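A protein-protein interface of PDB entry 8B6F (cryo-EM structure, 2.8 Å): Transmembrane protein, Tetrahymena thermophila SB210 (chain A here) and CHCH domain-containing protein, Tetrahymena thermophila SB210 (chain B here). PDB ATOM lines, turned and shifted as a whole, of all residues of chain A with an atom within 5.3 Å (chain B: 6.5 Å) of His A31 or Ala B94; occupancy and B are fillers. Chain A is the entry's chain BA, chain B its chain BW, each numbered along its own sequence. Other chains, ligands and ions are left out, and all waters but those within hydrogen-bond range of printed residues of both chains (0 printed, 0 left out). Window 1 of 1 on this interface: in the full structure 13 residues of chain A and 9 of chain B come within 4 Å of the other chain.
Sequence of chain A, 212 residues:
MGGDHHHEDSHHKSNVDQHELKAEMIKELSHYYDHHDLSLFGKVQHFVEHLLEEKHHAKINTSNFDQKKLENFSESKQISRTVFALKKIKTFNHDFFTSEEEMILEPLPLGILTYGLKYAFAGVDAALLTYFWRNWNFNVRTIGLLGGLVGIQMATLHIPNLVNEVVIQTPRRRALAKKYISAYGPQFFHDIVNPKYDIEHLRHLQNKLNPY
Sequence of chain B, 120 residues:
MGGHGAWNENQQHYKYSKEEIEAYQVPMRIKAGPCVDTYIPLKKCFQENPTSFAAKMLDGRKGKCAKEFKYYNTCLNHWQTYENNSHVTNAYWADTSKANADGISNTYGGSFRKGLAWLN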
ATOM      1  N   LYS A  27       7.557 -24.609 -16.169  1.00  0.00           N
ATOM      2  CA  LYS A  27       6.587 -23.675 -15.612  1.00  0.00           C
ATOM      3  C   LYS A  27       7.157 -22.263 -15.549  1.00  0.00           C
ATOM      4  O   LYS A  27       6.436 -21.284 -15.768  1.00  0.00           O
ATOM      5  CB  LYS A  27       6.158 -24.141 -14.220  1.00  0.00           C
ATOM      6  CG  LYS A  27       5.414 -25.470 -14.213  1.00  0.00           C
ATOM      7  CD  LYS A  27       5.266 -26.015 -12.797  1.00  0.00           C
ATOM      8  CE  LYS A  27       4.620 -27.393 -12.801  1.00  0.00           C
ATOM      9  NZ  LYS A  27       4.511 -27.963 -11.428  1.00  0.00           N
ATOM     10  N   GLU A  28       8.450 -22.139 -15.247  1.00  0.00           N
ATOM     11  CA  GLU A  28       9.052 -20.820 -15.099  1.00  0.00           C
ATOM     12  C   GLU A  28       9.325 -20.154 -16.442  1.00  0.00           C
ATOM     13  O   GLU A  28       9.164 -18.936 -16.573  1.00  0.00           O
ATOM     14  CB  GLU A  28      10.348 -20.931 -14.294  1.00  0.00           C
ATOM     15  CG  GLU A  28      10.955 -19.592 -13.904  1.00  0.00           C
ATOM     16  CD  GLU A  28      10.058 -18.791 -12.979  1.00  0.00           C
ATOM     17  OE1 GLU A  28       9.083 -19.362 -12.449  1.00  0.00           O
ATOM     18  OE2 GLU A  28      10.329 -17.587 -12.783  1.00  0.00           O
ATOM     19  N   LEU A  29       9.737 -20.925 -17.449  1.00  0.00           N
ATOM     20  CA  LEU A  29      10.296 -20.365 -18.674  1.00  0.00           C
ATOM     21  C   LEU A  29       9.430 -20.598 -19.903  1.00  0.00           C
ATOM     22  O   LEU A  29       9.866 -20.292 -21.017  1.00  0.00           O
ATOM     23  CB  LEU A  29      11.693 -20.939 -18.919  1.00  0.00           C
ATOM     24  CG  LEU A  29      12.726 -20.672 -17.824  1.00  0.00           C
ATOM     25  CD1 LEU A  29      14.015 -21.416 -18.120  1.00  0.00           C
ATOM     26  CD2 LEU A  29      12.990 -19.182 -17.680  1.00  0.00           C
ATOM     27  N   SER A  30       8.220 -21.135 -19.743  1.00  0.00           N
ATOM     28  CA  SER A  30       7.359 -21.315 -20.907  1.00  0.00           C
ATOM     29  C   SER A  30       7.040 -19.983 -21.576  1.00  0.00           C
ATOM     30  O   SER A  30       6.878 -19.927 -22.801  1.00  0.00           O
ATOM     31  CB  SER A  30       6.069 -22.027 -20.502  1.00  0.00           C
ATOM     32  OG  SER A  30       5.215 -22.206 -21.620  1.00  0.00           O
ATOM     33  N   HIS A  31       6.935 -18.909 -20.793  1.00  0.00           N
ATOM     34  CA  HIS A  31       6.526 -17.619 -21.336  1.00  0.00           C
ATOM     35  C   HIS A  31       7.466 -17.115 -22.423  1.00  0.00           C
ATOM     36  O   HIS A  31       7.059 -16.282 -23.239  1.00  0.00           O
ATOM     37  CB  HIS A  31       6.438 -16.579 -20.217  1.00  0.00           C
ATOM     38  CG  HIS A  31       5.534 -16.978 -19.091  1.00  0.00           C
ATOM     39  ND1 HIS A  31       5.386 -16.215 -17.953  1.00  0.00           N
ATOM     40  CD2 HIS A  31       4.728 -18.053 -18.930  1.00  0.00           C
ATOM     41  CE1 HIS A  31       4.531 -16.807 -17.137  1.00  0.00           C
ATOM     42  NE2 HIS A  31       4.118 -17.924 -17.706  1.00  0.00           N
ATOM     43  N   TYR A  32       8.708 -17.596 -22.455  1.00  0.00           N
ATOM     44  CA  TYR A  32       9.694 -17.111 -23.413  1.00  0.00           C
ATOM     45  C   TYR A  32       9.727 -17.942 -24.692  1.00  0.00           C
ATOM     46  O   TYR A  32       9.596 -17.396 -25.791  1.00  0.00           O
ATOM     47  CB  TYR A  32      11.081 -17.099 -22.765  1.00  0.00           C
ATOM     48  CG  TYR A  32      11.177 -16.236 -21.527  1.00  0.00           C
ATOM     49  CD1 TYR A  32      10.487 -15.036 -21.435  1.00  0.00           C
ATOM     50  CD2 TYR A  32      11.958 -16.626 -20.451  1.00  0.00           C
ATOM     51  CE1 TYR A  32      10.573 -14.249 -20.305  1.00  0.00           C
ATOM     52  CE2 TYR A  32      12.051 -15.847 -19.317  1.00  0.00           C
ATOM     53  CZ  TYR A  32      11.357 -14.660 -19.250  1.00  0.00           C
ATOM     54  OH  TYR A  32      11.447 -13.880 -18.122  1.00  0.00           O
ATOM     55  N   TYR A  33       9.906 -19.252 -24.568  1.00  0.00           N
ATOM     56  CA  TYR A  33      10.101 -20.118 -25.723  1.00  0.00           C
ATOM     57  C   TYR A  33       8.816 -20.767 -26.215  1.00  0.00           C
ATOM     58  O   TYR A  33       8.867 -21.547 -27.170  1.00  0.00           O
ATOM     59  CB  TYR A  33      11.125 -21.209 -25.395  1.00  0.00           C
ATOM     60  CG  TYR A  33      10.605 -22.297 -24.484  1.00  0.00           C
ATOM     61  CD1 TYR A  33      10.693 -22.177 -23.105  1.00  0.00           C
ATOM     62  CD2 TYR A  33      10.036 -23.451 -25.004  1.00  0.00           C
ATOM     63  CE1 TYR A  33      10.223 -23.172 -22.269  1.00  0.00           C
ATOM     64  CE2 TYR A  33       9.564 -24.451 -24.180  1.00  0.00           C
ATOM     65  CZ  TYR A  33       9.660 -24.307 -22.813  1.00  0.00           C
ATOM     66  OH  TYR A  33       9.191 -25.302 -21.991  1.00  0.00           O
ATOM     67  N   ASP A  34       7.672 -20.477 -25.594  1.00  0.00           N
ATOM     68  CA  ASP A  34       6.415 -21.076 -26.022  1.00  0.00           C
ATOM     69  C   ASP A  34       5.299 -20.041 -26.083  1.00  0.00           C
ATOM     70  O   ASP A  34       4.129 -20.371 -25.858  1.00  0.00           O
ATOM     71  CB  ASP A  34       6.020 -22.224 -25.090  1.00  0.00           C
ATOM     72  CG  ASP A  34       4.985 -23.144 -25.704  1.00  0.00           C
ATOM     73  OD1 ASP A  34       4.563 -22.884 -26.850  1.00  0.00           O
ATOM     74  OD2 ASP A  34       4.596 -24.129 -25.043  1.00  0.00           O
ATOM     75  N   HIS A  35       5.639 -18.790 -26.384  1.00  0.00           N
ATOM     76  CA  HIS A  35       4.667 -17.708 -26.465  1.00  0.00           C
ATOM     77  C   HIS A  35       4.799 -17.009 -27.809  1.00  0.00           C
ATOM     78  O   HIS A  35       5.907 -16.657 -28.223  1.00  0.00           O
ATOM     79  CB  HIS A  35       4.865 -16.697 -25.331  1.00  0.00           C
ATOM     80  CG  HIS A  35       4.008 -15.475 -25.460  1.00  0.00           C
ATOM     81  ND1 HIS A  35       4.413 -14.353 -26.150  1.00  0.00           N
ATOM     82  CD2 HIS A  35       2.766 -15.203 -24.994  1.00  0.00           C
ATOM     83  CE1 HIS A  35       3.459 -13.441 -26.103  1.00  0.00           C
ATOM     84  NE2 HIS A  35       2.449 -13.931 -25.407  1.00  0.00           N
ATOM     85  N   THR B  89      16.761 -11.242 -27.442  1.00  0.00           N
ATOM     86  CA  THR B  89      15.843 -10.282 -28.044  1.00  0.00           C
ATOM     87  C   THR B  89      14.448 -10.875 -28.192  1.00  0.00           C
ATOM     88  O   THR B  89      13.446 -10.193 -27.947  1.00  0.00           O
ATOM     89  CB  THR B  89      16.378  -9.831 -29.403  1.00  0.00           C
ATOM     90  OG1 THR B  89      17.688  -9.272 -29.244  1.00  0.00           O
ATOM     91  CG2 THR B  89      15.459  -8.791 -30.027  1.00  0.00           C
ATOM     92  N   ASN B  90      14.362 -12.142 -28.598  1.00  0.00           N
ATOM     93  CA  ASN B  90      13.059 -12.787 -28.727  1.00  0.00           C
ATOM     94  C   ASN B  90      12.375 -12.931 -27.375  1.00  0.00           C
ATOM     95  O   ASN B  90      11.158 -12.745 -27.268  1.00  0.00           O
ATOM     96  CB  ASN B  90      13.211 -14.149 -29.401  1.00  0.00           C
ATOM     97  CG  ASN B  90      13.447 -14.036 -30.893  1.00  0.00           C
ATOM     98  OD1 ASN B  90      13.835 -12.983 -31.393  1.00  0.00           O
ATOM     99  ND2 ASN B  90      13.212 -15.125 -31.614  1.00  0.00           N
ATOM    100  N   ALA B  91      13.133 -13.262 -26.327  1.00  0.00           N
ATOM    101  CA  ALA B  91      12.535 -13.358 -25.000  1.00  0.00           C
ATOM    102  C   ALA B  91      11.995 -12.008 -24.547  1.00  0.00           C
ATOM    103  O   ALA B  91      10.888 -11.924 -24.004  1.00  0.00           O
ATOM    104  CB  ALA B  91      13.560 -13.889 -23.998  1.00  0.00           C
ATOM    105  N   TYR B  92      12.765 -10.939 -24.757  1.00  0.00           N
ATOM    106  CA  TYR B  92      12.293  -9.607 -24.396  1.00  0.00           C
ATOM    107  C   TYR B  92      11.062  -9.223 -25.205  1.00  0.00           C
ATOM    108  O   TYR B  92      10.123  -8.620 -24.674  1.00  0.00           O
ATOM    109  CB  TYR B  92      13.408  -8.581 -24.589  1.00  0.00           C
ATOM    110  CG  TYR B  92      14.206  -8.328 -23.334  1.00  0.00           C
ATOM    111  CD1 TYR B  92      15.278  -9.139 -22.992  1.00  0.00           C
ATOM    112  CD2 TYR B  92      13.877  -7.281 -22.485  1.00  0.00           C
ATOM    113  CE1 TYR B  92      16.004  -8.910 -21.840  1.00  0.00           C
ATOM    114  CE2 TYR B  92      14.594  -7.044 -21.334  1.00  0.00           C
ATOM    115  CZ  TYR B  92      15.657  -7.862 -21.016  1.00  0.00           C
ATOM    116  OH  TYR B  92      16.372  -7.624 -19.869  1.00  0.00           O
ATOM    117  N   TRP B  93      11.056  -9.553 -26.496  1.00  0.00           N
ATOM    118  CA  TRP B  93       9.889  -9.281 -27.328  1.00  0.00           C
ATOM    119  C   TRP B  93       8.668 -10.029 -26.814  1.00  0.00           C
ATOM    120  O   TRP B  93       7.570  -9.465 -26.736  1.00  0.00           O
ATOM    121  CB  TRP B  93      10.184  -9.664 -28.779  1.00  0.00           C
ATOM    122  CG  TRP B  93       9.143  -9.209 -29.758  1.00  0.00           C
ATOM    123  CD1 TRP B  93       7.971  -9.837 -30.061  1.00  0.00           C
ATOM    124  CD2 TRP B  93       9.185  -8.025 -30.566  1.00  0.00           C
ATOM    125  NE1 TRP B  93       7.279  -9.117 -31.005  1.00  0.00           N
ATOM    126  CE2 TRP B  93       8.004  -8.001 -31.332  1.00  0.00           C
ATOM    127  CE3 TRP B  93      10.106  -6.984 -30.713  1.00  0.00           C
ATOM    128  CZ2 TRP B  93       7.719  -6.976 -32.231  1.00  0.00           C
ATOM    129  CZ3 TRP B  93       9.823  -5.967 -31.608  1.00  0.00           C
ATOM    130  CH2 TRP B  93       8.638  -5.971 -32.356  1.00  0.00           C
ATOM    131  N   ALA B  94       8.842 -11.298 -26.446  1.00  0.00           N
ATOM    132  CA  ALA B  94       7.719 -12.100 -25.971  1.00  0.00           C
ATOM    133  C   ALA B  94       7.141 -11.541 -24.677  1.00  0.00           C
ATOM    134  O   ALA B  94       5.918 -11.423 -24.534  1.00  0.00           O
ATOM    135  CB  ALA B  94       8.164 -13.549 -25.778  1.00  0.00           C
ATOM    136  N   ASP B  95       7.999 -11.193 -23.717  1.00  0.00           N
ATOM    137  CA  ASP B  95       7.523 -10.613 -22.457  1.00  0.00           C
ATOM    138  C   ASP B  95       8.594  -9.648 -21.944  1.00  0.00           C
ATOM    139  O   ASP B  95       9.531 -10.051 -21.253  1.00  0.00           O
ATOM    140  CB  ASP B  95       7.210 -11.696 -21.436  1.00  0.00           C
ATOM    141  CG  ASP B  95       6.338 -11.192 -20.304  1.00  0.00           C
ATOM    142  OD1 ASP B  95       6.435  -9.994 -19.964  1.00  0.00           O
ATOM    143  OD2 ASP B  95       5.550 -11.991 -19.757  1.00  0.00           O
ATOM    144  N   THR B  96       8.437  -8.370 -22.294  1.00  0.00           N
ATOM    145  CA  THR B  96       9.333  -7.343 -21.770  1.00  0.00           C
ATOM    146  C   THR B  96       9.177  -7.185 -20.262  1.00  0.00           C
ATOM    147  O   THR B  96      10.175  -7.059 -19.541  1.00  0.00           O
ATOM    148  CB  THR B  96       9.068  -6.011 -22.471  1.00  0.00           C
ATOM    149  OG1 THR B  96       9.179  -6.182 -23.890  1.00  0.00           O
ATOM    150  CG2 THR B  96      10.067  -4.954 -22.017  1.00  0.00           C
ATOM    151  N   LYS B  98       8.122  -9.299 -17.847  1.00  0.00           N
ATOM    152  CA  LYS B  98       8.718 -10.394 -17.091  1.00  0.00           C
ATOM    153  C   LYS B  98      10.234 -10.391 -17.224  1.00  0.00           C
ATOM    154  O   LYS B  98      10.948 -10.668 -16.254  1.00  0.00           O
ATOM    155  CB  LYS B  98       8.149 -11.733 -17.556  1.00  0.00           C
ATOM    156  CG  LYS B  98       8.625 -12.917 -16.724  1.00  0.00           C
ATOM    157  CD  LYS B  98       8.138 -14.238 -17.297  1.00  0.00           C
ATOM    158  CE  LYS B  98       8.714 -15.412 -16.523  1.00  0.00           C
ATOM    159  NZ  LYS B  98       8.358 -16.720 -17.140  1.00  0.00           N
ATOM    160  N   LYS B 114      10.132  -1.777 -27.640  1.00  0.00           N
ATOM    161  CA  LYS B 114       9.380  -2.321 -28.759  1.00  0.00           C
ATOM    162  C   LYS B 114       8.560  -1.229 -29.433  1.00  0.00           C
ATOM    163  O   LYS B 114       8.080  -0.291 -28.791  1.00  0.00           O
ATOM    164  CB  LYS B 114       8.466  -3.453 -28.288  1.00  0.00           C
ATOM    165  CG  LYS B 114       7.611  -4.052 -29.394  1.00  0.00           C
ATOM    166  CD  LYS B 114       7.208  -5.486 -29.083  1.00  0.00           C
ATOM    167  CE  LYS B 114       6.371  -5.579 -27.819  1.00  0.00           C
ATOM    168  NZ  LYS B 114       5.952  -6.982 -27.542  1.00  0.00           N
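O of Glu A28 sits at hydrogen-bond distance from NZ of Lys B98, 2.4 Å away. A ring nitrogen (ND1) of His A31 sits at hydrogen-bond distance from the side-chain amino group (NZ) of Lys B98 (3.1 Å).
Of the printed residues of chain B, Glu A28 touches Lys B98 (2.4 Å). Printed residues of chain B within 4 Å of His A31: Ala B94 (3.9 Å) and Lys B98 (3.1 Å). Of the printed residues of chain B, Tyr A32 touches Lys B98 (3.3 Å). Tyr A33 touches none of the printed residues of chain B. Of the printed residues of chain B, His A35 touches Ala B94 (3.5 Å). Of chain A, only His A31 and His A35 come within 4 Å of Ala B94. Printed residues of chain A within 4 Å of Lys B98: Glu A28 (2.4 Å), His A31 (3.1 Å) and Tyr A32 (3.3 Å). The nearest residue of chain B that does not touch His A31 is Asp B95 (4.6 Å).
OD1 of Asp B95 sits at hydrogen-bond distance from N of Lys B98.
Ala B94 touches His A31. CG of Lys B98 touches OH of Tyr A32 (3.3 Å). CE1 of His A35 touches O of Ala B94 (3.5 Å).
Printed residues of chain B that touch a printed residue of chain A: Ala B94 and Lys B98. Of the 9 printed residues of chain A, 4 touch a printed residue of chain B. Hydrophobic or aromatic side chains of chain A that line the printed part of chain B: His A31, Tyr A32 and His A35. Among the printed residues, no Asp or Glu carboxylate lies within 4 Å of a Lys or Arg side-chain nitrogen of the other chain.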
